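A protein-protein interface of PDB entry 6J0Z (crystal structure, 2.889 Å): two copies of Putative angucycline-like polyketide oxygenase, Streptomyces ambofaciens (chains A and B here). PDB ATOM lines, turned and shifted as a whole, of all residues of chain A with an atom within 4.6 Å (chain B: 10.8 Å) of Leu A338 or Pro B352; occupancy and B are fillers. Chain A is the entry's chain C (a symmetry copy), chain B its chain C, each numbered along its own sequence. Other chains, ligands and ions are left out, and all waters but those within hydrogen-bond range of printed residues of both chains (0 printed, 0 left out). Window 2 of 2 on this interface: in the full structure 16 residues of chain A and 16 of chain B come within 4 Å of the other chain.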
ATOM      1  N   THR A 173      23.406  36.573 -12.114  1.00  0.00           N
ATOM      2  CA  THR A 173      23.198  35.360 -11.336  1.00  0.00           C
ATOM      3  C   THR A 173      24.508  34.865 -10.750  1.00  0.00           C
ATOM      4  O   THR A 173      25.543  34.878 -11.425  1.00  0.00           O
ATOM      5  CB  THR A 173      22.590  34.282 -12.233  1.00  0.00           C
ATOM      6  OG1 THR A 173      21.334  34.741 -12.738  1.00  0.00           O
ATOM      7  CG2 THR A 173      22.374  32.980 -11.484  1.00  0.00           C
ATOM      8  N   ASP A 261      28.459  29.398 -15.302  1.00  0.00           N
ATOM      9  CA  ASP A 261      27.077  29.606 -15.700  1.00  0.00           C
ATOM     10  C   ASP A 261      26.553  30.930 -15.165  1.00  0.00           C
ATOM     11  O   ASP A 261      25.335  31.101 -15.024  1.00  0.00           O
ATOM     12  CB  ASP A 261      26.183  28.436 -15.270  1.00  0.00           C
ATOM     13  CG  ASP A 261      26.066  28.277 -13.767  1.00  0.00           C
ATOM     14  OD1 ASP A 261      26.912  28.811 -13.019  1.00  0.00           O
ATOM     15  OD2 ASP A 261      25.112  27.587 -13.344  1.00  0.00           O
ATOM     16  N   SER A 263      24.993  34.251 -15.432  1.00  0.00           N
ATOM     17  CA  SER A 263      24.151  34.962 -16.384  1.00  0.00           C
ATOM     18  C   SER A 263      23.976  36.381 -15.867  1.00  0.00           C
ATOM     19  O   SER A 263      23.485  36.579 -14.751  1.00  0.00           O
ATOM     20  CB  SER A 263      22.790  34.283 -16.550  1.00  0.00           C
ATOM     21  OG  SER A 263      21.973  34.438 -15.407  1.00  0.00           O
ATOM     22  N   LEU A 334      18.580  34.228 -20.763  1.00  0.00           N
ATOM     23  CA  LEU A 334      19.362  33.854 -19.587  1.00  0.00           C
ATOM     24  C   LEU A 334      18.597  32.838 -18.748  1.00  0.00           C
ATOM     25  O   LEU A 334      19.169  31.840 -18.291  1.00  0.00           O
ATOM     26  CB  LEU A 334      19.728  35.083 -18.757  1.00  0.00           C
ATOM     27  CG  LEU A 334      20.911  35.992 -19.134  1.00  0.00           C
ATOM     28  CD1 LEU A 334      20.757  36.583 -20.527  1.00  0.00           C
ATOM     29  CD2 LEU A 334      21.069  37.094 -18.079  1.00  0.00           C
ATOM     30  N   THR A 335      17.284  33.047 -18.593  1.00  0.00           N
ATOM     31  CA  THR A 335      16.449  32.123 -17.830  1.00  0.00           C
ATOM     32  C   THR A 335      16.403  30.749 -18.492  1.00  0.00           C
ATOM     33  O   THR A 335      16.515  29.717 -17.818  1.00  0.00           O
ATOM     34  CB  THR A 335      15.042  32.711 -17.690  1.00  0.00           C
ATOM     35  OG1 THR A 335      15.120  34.037 -17.155  1.00  0.00           O
ATOM     36  CG2 THR A 335      14.173  31.878 -16.773  1.00  0.00           C
ATOM     37  N   ASN A 336      16.278  30.715 -19.815  1.00  0.00           N
ATOM     38  CA  ASN A 336      16.147  29.432 -20.494  1.00  0.00           C
ATOM     39  C   ASN A 336      17.464  28.671 -20.565  1.00  0.00           C
ATOM     40  O   ASN A 336      17.457  27.438 -20.496  1.00  0.00           O
ATOM     41  CB  ASN A 336      15.569  29.634 -21.891  1.00  0.00           C
ATOM     42  CG  ASN A 336      14.103  30.013 -21.857  1.00  0.00           C
ATOM     43  OD1 ASN A 336      13.356  29.584 -20.974  1.00  0.00           O
ATOM     44  ND2 ASN A 336      13.683  30.829 -22.818  1.00  0.00           N
ATOM     45  N   THR A 337      18.595  29.362 -20.715  1.00  0.00           N
ATOM     46  CA  THR A 337      19.865  28.654 -20.696  1.00  0.00           C
ATOM     47  C   THR A 337      20.171  28.145 -19.295  1.00  0.00           C
ATOM     48  O   THR A 337      20.610  26.995 -19.136  1.00  0.00           O
ATOM     49  CB  THR A 337      20.984  29.547 -21.216  1.00  0.00           C
ATOM     50  OG1 THR A 337      21.030  30.738 -20.432  1.00  0.00           O
ATOM     51  CG2 THR A 337      20.732  29.900 -22.681  1.00  0.00           C
ATOM     52  N   LEU A 338      19.905  28.966 -18.264  1.00  0.00           N
ATOM     53  CA  LEU A 338      19.931  28.463 -16.893  1.00  0.00           C
ATOM     54  C   LEU A 338      19.111  27.188 -16.784  1.00  0.00           C
ATOM     55  O   LEU A 338      19.582  26.186 -16.239  1.00  0.00           O
ATOM     56  CB  LEU A 338      19.401  29.524 -15.916  1.00  0.00           C
ATOM     57  CG  LEU A 338      20.225  30.739 -15.452  1.00  0.00           C
ATOM     58  CD1 LEU A 338      19.349  31.702 -14.656  1.00  0.00           C
ATOM     59  CD2 LEU A 338      21.454  30.321 -14.640  1.00  0.00           C
ATOM     60  N   ALA A 339      17.892  27.201 -17.335  1.00  0.00           N
ATOM     61  CA  ALA A 339      16.990  26.059 -17.209  1.00  0.00           C
ATOM     62  C   ALA A 339      17.562  24.819 -17.884  1.00  0.00           C
ATOM     63  O   ALA A 339      17.667  23.749 -17.266  1.00  0.00           O
ATOM     64  CB  ALA A 339      15.626  26.411 -17.795  1.00  0.00           C
ATOM     65  N   GLN A 340      17.901  24.944 -19.166  1.00  0.00           N
ATOM     66  CA  GLN A 340      18.500  23.849 -19.910  1.00  0.00           C
ATOM     67  C   GLN A 340      19.662  23.242 -19.151  1.00  0.00           C
ATOM     68  O   GLN A 340      19.727  22.022 -18.977  1.00  0.00           O
ATOM     69  CB  GLN A 340      18.989  24.354 -21.260  1.00  0.00           C
ATOM     70  CG  GLN A 340      18.028  24.259 -22.386  1.00  0.00           C
ATOM     71  CD  GLN A 340      18.771  24.165 -23.669  1.00  0.00           C
ATOM     72  OE1 GLN A 340      20.000  24.171 -23.669  1.00  0.00           O
ATOM     73  NE2 GLN A 340      18.057  24.072 -24.772  1.00  0.00           N
ATOM     74  N   ARG A 341      20.590  24.075 -18.684  1.00  0.00           N
ATOM     75  CA  ARG A 341      21.815  23.525 -18.127  1.00  0.00           C
ATOM     76  C   ARG A 341      21.617  23.008 -16.715  1.00  0.00           C
ATOM     77  O   ARG A 341      22.357  22.121 -16.292  1.00  0.00           O
ATOM     78  CB  ARG A 341      22.926  24.569 -18.193  1.00  0.00           C
ATOM     79  CG  ARG A 341      23.122  25.162 -19.603  1.00  0.00           C
ATOM     80  CD  ARG A 341      23.771  24.208 -20.614  1.00  0.00           C
ATOM     81  NE  ARG A 341      22.792  23.532 -21.457  1.00  0.00           N
ATOM     82  CZ  ARG A 341      23.102  22.720 -22.462  1.00  0.00           C
ATOM     83  NH1 ARG A 341      24.373  22.486 -22.762  1.00  0.00           N
ATOM     84  NH2 ARG A 341      22.137  22.142 -23.165  1.00  0.00           N
ATOM     85  N   ILE A 342      20.620  23.498 -15.988  1.00  0.00           N
ATOM     86  CA  ILE A 342      20.268  22.820 -14.750  1.00  0.00           C
ATOM     87  C   ILE A 342      19.798  21.405 -15.042  1.00  0.00           C
ATOM     88  O   ILE A 342      20.240  20.433 -14.412  1.00  0.00           O
ATOM     89  CB  ILE A 342      19.188  23.616 -13.997  1.00  0.00           C
ATOM     90  CG1 ILE A 342      19.804  24.837 -13.312  1.00  0.00           C
ATOM     91  CG2 ILE A 342      18.491  22.708 -13.000  1.00  0.00           C
ATOM     92  CD1 ILE A 342      20.945  24.484 -12.365  1.00  0.00           C
ATOM     93  N   GLY B  78       4.243  21.222  -8.703  1.00  0.00           N
ATOM     94  CA  GLY B  78       5.428  21.983  -8.355  1.00  0.00           C
ATOM     95  C   GLY B  78       5.108  23.410  -7.952  1.00  0.00           C
ATOM     96  O   GLY B  78       5.989  24.272  -7.952  1.00  0.00           O
ATOM     97  N   VAL B  80       2.682  25.217  -9.602  1.00  0.00           N
ATOM     98  CA  VAL B  80       2.043  25.886 -10.737  1.00  0.00           C
ATOM     99  C   VAL B  80       0.602  25.426 -10.772  1.00  0.00           C
ATOM    100  O   VAL B  80       0.344  24.226 -11.000  1.00  0.00           O
ATOM    101  CB  VAL B  80       2.774  25.576 -12.054  1.00  0.00           C
ATOM    102  CG1 VAL B  80       2.130  26.315 -13.226  1.00  0.00           C
ATOM    103  CG2 VAL B  80       4.236  25.944 -11.945  1.00  0.00           C
ATOM    104  N   ARG B 197      10.091  32.368  -0.729  1.00  0.00           N
ATOM    105  CA  ARG B 197      11.328  31.587  -0.730  1.00  0.00           C
ATOM    106  C   ARG B 197      12.450  32.550  -0.360  1.00  0.00           C
ATOM    107  O   ARG B 197      13.216  33.024  -1.199  1.00  0.00           O
ATOM    108  CB  ARG B 197      11.556  30.926  -2.084  1.00  0.00           C
ATOM    109  CG  ARG B 197      10.354  30.137  -2.546  1.00  0.00           C
ATOM    110  CD  ARG B 197      10.477  29.582  -3.948  1.00  0.00           C
ATOM    111  NE  ARG B 197       9.289  28.796  -4.281  1.00  0.00           N
ATOM    112  CZ  ARG B 197       8.216  29.277  -4.906  1.00  0.00           C
ATOM    113  NH1 ARG B 197       8.184  30.550  -5.288  1.00  0.00           N
ATOM    114  NH2 ARG B 197       7.178  28.486  -5.166  1.00  0.00           N
ATOM    115  N   ILE B 342      11.578  19.822  -6.127  1.00  0.00           N
ATOM    116  CA  ILE B 342      12.721  20.582  -6.609  1.00  0.00           C
ATOM    117  C   ILE B 342      12.258  21.900  -7.208  1.00  0.00           C
ATOM    118  O   ILE B 342      12.795  22.974  -6.903  1.00  0.00           O
ATOM    119  CB  ILE B 342      13.512  19.756  -7.637  1.00  0.00           C
ATOM    120  CG1 ILE B 342      14.350  18.688  -6.932  1.00  0.00           C
ATOM    121  CG2 ILE B 342      14.377  20.681  -8.474  1.00  0.00           C
ATOM    122  CD1 ILE B 342      15.296  19.259  -5.883  1.00  0.00           C
ATOM    123  N   LEU B 343      11.206  21.837  -8.009  1.00  0.00           N
ATOM    124  CA  LEU B 343      10.719  22.987  -8.742  1.00  0.00           C
ATOM    125  C   LEU B 343       9.887  23.909  -7.875  1.00  0.00           C
ATOM    126  O   LEU B 343       9.530  25.002  -8.311  1.00  0.00           O
ATOM    127  CB  LEU B 343       9.886  22.470  -9.897  1.00  0.00           C
ATOM    128  CG  LEU B 343       9.429  23.333 -11.041  1.00  0.00           C
ATOM    129  CD1 LEU B 343       9.636  22.454 -12.261  1.00  0.00           C
ATOM    130  CD2 LEU B 343       7.973  23.692 -10.796  1.00  0.00           C
ATOM    131  N   TYR B 344       9.545  23.475  -6.673  1.00  0.00           N
ATOM    132  CA  TYR B 344       8.689  24.230  -5.781  1.00  0.00           C
ATOM    133  C   TYR B 344       9.449  24.775  -4.576  1.00  0.00           C
ATOM    134  O   TYR B 344       9.409  25.978  -4.305  1.00  0.00           O
ATOM    135  CB  TYR B 344       7.532  23.343  -5.331  1.00  0.00           C
ATOM    136  CG  TYR B 344       6.542  24.079  -4.478  1.00  0.00           C
ATOM    137  CD1 TYR B 344       5.820  25.135  -4.990  1.00  0.00           C
ATOM    138  CD2 TYR B 344       6.346  23.730  -3.155  1.00  0.00           C
ATOM    139  CE1 TYR B 344       4.914  25.821  -4.221  1.00  0.00           C
ATOM    140  CE2 TYR B 344       5.445  24.408  -2.365  1.00  0.00           C
ATOM    141  CZ  TYR B 344       4.727  25.455  -2.902  1.00  0.00           C
ATOM    142  OH  TYR B 344       3.822  26.137  -2.127  1.00  0.00           O
ATOM    143  N   GLY B 346      12.804  24.691  -4.121  1.00  0.00           N
ATOM    144  CA  GLY B 346      14.129  25.211  -4.520  1.00  0.00           C
ATOM    145  C   GLY B 346      14.188  26.728  -4.574  1.00  0.00           C
ATOM    146  O   GLY B 346      13.114  27.356  -4.647  1.00  0.00           O
ATOM    147  N   GLY B 347      15.401  27.297  -4.541  1.00  0.00           N
ATOM    148  CA  GLY B 347      15.538  28.732  -4.607  1.00  0.00           C
ATOM    149  C   GLY B 347      15.657  29.274  -6.014  1.00  0.00           C
ATOM    150  O   GLY B 347      14.867  28.948  -6.905  1.00  0.00           O
ATOM    151  N   ASP B 348      16.680  30.105  -6.202  1.00  0.00           N
ATOM    152  CA  ASP B 348      16.957  30.854  -7.452  1.00  0.00           C
ATOM    153  C   ASP B 348      17.468  29.988  -8.613  1.00  0.00           C
ATOM    154  O   ASP B 348      17.729  30.542  -9.688  1.00  0.00           O
ATOM    155  CB  ASP B 348      18.060  31.842  -7.123  1.00  0.00           C
ATOM    156  CG  ASP B 348      18.273  32.858  -8.208  1.00  0.00           C
ATOM    157  OD1 ASP B 348      17.518  32.885  -9.195  1.00  0.00           O
ATOM    158  OD2 ASP B 348      19.177  33.702  -8.015  1.00  0.00           O
ATOM    159  N   GLU B 349      17.594  28.670  -8.439  1.00  0.00           N
ATOM    160  CA  GLU B 349      18.133  27.818  -9.493  1.00  0.00           C
ATOM    161  C   GLU B 349      16.915  27.272 -10.213  1.00  0.00           C
ATOM    162  O   GLU B 349      16.981  26.995 -11.417  1.00  0.00           O
ATOM    163  CB  GLU B 349      18.968  26.650  -8.966  1.00  0.00           C
ATOM    164  CG  GLU B 349      20.328  27.007  -8.429  1.00  0.00           C
ATOM    165  CD  GLU B 349      21.024  25.794  -7.844  1.00  0.00           C
ATOM    166  OE1 GLU B 349      20.535  24.666  -8.063  1.00  0.00           O
ATOM    167  OE2 GLU B 349      22.053  25.965  -7.162  1.00  0.00           O
ATOM    168  N   ILE B 350      15.806  27.114  -9.494  1.00  0.00           N
ATOM    169  CA  ILE B 350      14.593  26.564 -10.067  1.00  0.00           C
ATOM    170  C   ILE B 350      13.619  27.695 -10.424  1.00  0.00           C
ATOM    171  O   ILE B 350      12.462  27.338 -10.804  1.00  0.00           O
ATOM    172  CB  ILE B 350      13.977  25.486  -9.150  1.00  0.00           C
ATOM    173  CG1 ILE B 350      13.709  26.040  -7.761  1.00  0.00           C
ATOM    174  CG2 ILE B 350      14.894  24.266  -9.051  1.00  0.00           C
ATOM    175  CD1 ILE B 350      12.315  26.463  -7.508  1.00  0.00           C
ATOM    176  N   THR B 351      14.019  28.977 -10.260  1.00  0.00           N
ATOM    177  CA  THR B 351      13.100  30.025 -10.781  1.00  0.00           C
ATOM    178  C   THR B 351      12.789  29.747 -12.262  1.00  0.00           C
ATOM    179  O   THR B 351      11.596  29.812 -12.623  1.00  0.00           O
ATOM    180  CB  THR B 351      13.707  31.401 -10.482  1.00  0.00           C
ATOM    181  OG1 THR B 351      13.861  31.594  -9.075  1.00  0.00           O
ATOM    182  CG2 THR B 351      12.839  32.540 -10.959  1.00  0.00           C
ATOM    183  N   PRO B 352      13.780  29.444 -13.138  1.00  0.00           N
ATOM    184  CA  PRO B 352      13.516  29.164 -14.562  1.00  0.00           C
ATOM    185  C   PRO B 352      12.592  27.978 -14.724  1.00  0.00           C
ATOM    186  O   PRO B 352      11.827  27.936 -15.695  1.00  0.00           O
ATOM    187  CB  PRO B 352      14.900  28.899 -15.169  1.00  0.00           C
ATOM    188  CG  PRO B 352      15.867  29.488 -14.200  1.00  0.00           C
ATOM    189  CD  PRO B 352      15.210  29.370 -12.837  1.00  0.00           C
ATOM    190  N   MET B 353      12.701  27.086 -13.750  1.00  0.00           N
ATOM    191  CA  MET B 353      11.828  25.914 -13.837  1.00  0.00           C
ATOM    192  C   MET B 353      10.359  26.295 -13.729  1.00  0.00           C
ATOM    193  O   MET B 353       9.534  25.882 -14.561  1.00  0.00           O
ATOM    194  CB  MET B 353      12.181  24.911 -12.744  1.00  0.00           C
ATOM    195  CG  MET B 353      13.613  24.487 -12.721  1.00  0.00           C
ATOM    196  SD  MET B 353      13.968  23.478 -14.140  1.00  0.00           S
ATOM    197  CE  MET B 353      15.242  24.443 -14.910  1.00  0.00           C
ATOM    198  N   ARG B 354      10.053  27.070 -12.705  1.00  0.00           N
ATOM    199  CA  ARG B 354       8.660  27.503 -12.500  1.00  0.00           C
ATOM    200  C   ARG B 354       8.225  28.276 -13.732  1.00  0.00           C
ATOM    201  O   ARG B 354       7.092  28.101 -14.160  1.00  0.00           O
ATOM    202  CB  ARG B 354       8.594  28.380 -11.257  1.00  0.00           C
ATOM    203  CG  ARG B 354       8.141  27.629 -10.020  1.00  0.00           C
ATOM    204  CD  ARG B 354       9.170  27.841  -8.952  1.00  0.00           C
ATOM    205  NE  ARG B 354       9.432  29.253  -8.873  1.00  0.00           N
ATOM    206  CZ  ARG B 354      10.116  29.804  -7.897  1.00  0.00           C
ATOM    207  NH1 ARG B 354      10.539  29.062  -6.893  1.00  0.00           N
ATOM    208  NH2 ARG B 354      10.344  31.098  -7.913  1.00  0.00           N
ATOM    209  N   GLU B 355       9.113  29.106 -14.266  1.00  0.00           N
ATOM    210  CA  GLU B 355       8.753  29.866 -15.451  1.00  0.00           C
ATOM    211  C   GLU B 355       8.414  28.934 -16.602  1.00  0.00           C
ATOM    212  O   GLU B 355       7.337  29.038 -17.203  1.00  0.00           O
ATOM    213  CB  GLU B 355       9.879  30.816 -15.825  1.00  0.00           C
ATOM    214  CG  GLU B 355       9.493  31.815 -16.894  1.00  0.00           C
ATOM    215  CD  GLU B 355      10.532  32.903 -17.067  1.00  0.00           C
ATOM    216  OE1 GLU B 355      11.418  33.027 -16.199  1.00  0.00           O
ATOM    217  OE2 GLU B 355      10.466  33.639 -18.071  1.00  0.00           O
ATOM    218  N   VAL B 356       9.294  27.976 -16.880  1.00  0.00           N
ATOM    219  CA  VAL B 356       9.136  27.157 -18.074  1.00  0.00           C
ATOM    220  C   VAL B 356       7.869  26.329 -17.978  1.00  0.00           C
ATOM    221  O   VAL B 356       7.079  26.268 -18.926  1.00  0.00           O
ATOM    222  CB  VAL B 356      10.370  26.267 -18.290  1.00  0.00           C
ATOM    223  CG1 VAL B 356      10.094  25.266 -19.397  1.00  0.00           C
ATOM    224  CG2 VAL B 356      11.584  27.115 -18.643  1.00  0.00           C
ATOM    225  N   LEU B 357       7.652  25.679 -16.829  1.00  0.00           N
ATOM    226  CA  LEU B 357       6.442  24.885 -16.686  1.00  0.00           C
ATOM    227  C   LEU B 357       5.214  25.785 -16.712  1.00  0.00           C
ATOM    228  O   LEU B 357       4.222  25.425 -17.347  1.00  0.00           O
ATOM    229  CB  LEU B 357       6.495  24.001 -15.436  1.00  0.00           C
ATOM    230  CG  LEU B 357       7.467  22.839 -15.176  1.00  0.00           C
ATOM    231  CD1 LEU B 357       6.909  22.101 -13.999  1.00  0.00           C
ATOM    232  CD2 LEU B 357       7.660  21.853 -16.320  1.00  0.00           C
ATOM    233  N   ALA B 358       5.248  26.953 -16.056  1.00  0.00           N
ATOM    234  CA  ALA B 358       4.143  27.892 -16.195  1.00  0.00           C
ATOM    235  C   ALA B 358       3.800  28.149 -17.652  1.00  0.00           C
ATOM    236  O   ALA B 358       2.627  28.210 -18.025  1.00  0.00           O
ATOM    237  CB  ALA B 358       4.454  29.202 -15.461  1.00  0.00           C
ATOM    238  N   GLU B 359       4.817  28.246 -18.497  1.00  0.00           N
ATOM    239  CA  GLU B 359       4.577  28.448 -19.918  1.00  0.00           C
ATOM    240  C   GLU B 359       4.013  27.185 -20.576  1.00  0.00           C
ATOM    241  O   GLU B 359       3.043  27.252 -21.342  1.00  0.00           O
ATOM    242  CB  GLU B 359       5.879  28.912 -20.561  1.00  0.00           C
ATOM    243  CG  GLU B 359       6.422  30.221 -19.943  1.00  0.00           C
ATOM    244  CD  GLU B 359       7.825  30.609 -20.405  1.00  0.00           C
ATOM    245  OE1 GLU B 359       8.626  29.721 -20.724  1.00  0.00           O
ATOM    246  OE2 GLU B 359       8.138  31.814 -20.476  1.00  0.00           O
ATOM    247  N   LEU B 360       4.569  26.022 -20.231  1.00  0.00           N
ATOM    248  CA  LEU B 360       4.116  24.763 -20.809  1.00  0.00           C
ATOM    249  C   LEU B 360       2.682  24.428 -20.418  1.00  0.00           C
ATOM    250  O   LEU B 360       1.970  23.790 -21.205  1.00  0.00           O
ATOM    251  CB  LEU B 360       5.063  23.642 -20.381  1.00  0.00           C
ATOM    252  CG  LEU B 360       6.496  23.726 -20.905  1.00  0.00           C
ATOM    253  CD1 LEU B 360       7.364  22.641 -20.286  1.00  0.00           C
ATOM    254  CD2 LEU B 360       6.475  23.619 -22.412  1.00  0.00           C
ATOM    255  N   MET B 361       2.243  24.844 -19.219  1.00  0.00           N
ATOM    256  CA  MET B 361       0.867  24.619 -18.781  1.00  0.00           C
ATOM    257  C   MET B 361      -0.141  25.431 -19.570  1.00  0.00           C
ATOM    258  O   MET B 361      -1.344  25.165 -19.451  1.00  0.00           O
ATOM    259  CB  MET B 361       0.633  24.980 -17.312  1.00  0.00           C
ATOM    260  CG  MET B 361       1.467  24.321 -16.248  1.00  0.00           C
ATOM    261  SD  MET B 361       1.865  22.595 -16.472  1.00  0.00           S
ATOM    262  CE  MET B 361       0.291  21.841 -16.813  1.00  0.00           C
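Thr A335 touches Pro B352. Glu B355 touches Thr A335. Val B356 touches Asn A336. Pro B352 touches Leu A338. Pro B352 touches Ala A339 (CB to CB, 3.7 Å). CA of Ala A339 touches CE of Met B353, 3.3 Å away.
Leu A338 touches one residue of chain B. Of chain A, only Thr A335, Leu A338 and Ala A339 come within 4 Å of Pro B352. No residue of chain B comes within 4 Å of Ser A263. Thr A335 touches just these residues of chain B: Pro B352 (3.2 Å) and Glu B355 (3.0 Å). No residue of chain B comes within 4 Å of Thr A337. Printed residues of chain B within 4 Å of Ala A339: Pro B352 (3.7 Å) and Met B353 (3.3 Å). No residue of chain B comes within 4 Å of Ile A342. Printed residues of chain A within 4 Å of Val B356: Asn A336. Of the printed residues of chain A, Met B353 touches Ala A339. Printed residues of chain B within 4 Å of Asn A336: Val B356. Gly B347 touches none of the printed residues of chain A. Gly B78 touches none of the printed residues of chain A. The nearest residue of chain B that does not touch Leu A338 is Met B353 (4.9 Å).
Hydrophobic or aromatic side chains of chain A that line the printed part of chain B: Leu A338 and Ala A339. Of the 22 printed residues of chain B, 4 touch a printed residue of chain A. Printed residues of chain B that touch a printed residue of chain A: Pro B352, Met B353, Glu B355 and Val B356. Hydrophobic or aromatic side chains of chain B within 4 Å of the printed part of chain A: Pro B352, Met B353 and Val B356.
1 position is printed for both chains. Of the 6 pairs that touch across the chains among the printed residues, none has its exchanged pair printed and touching as well.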
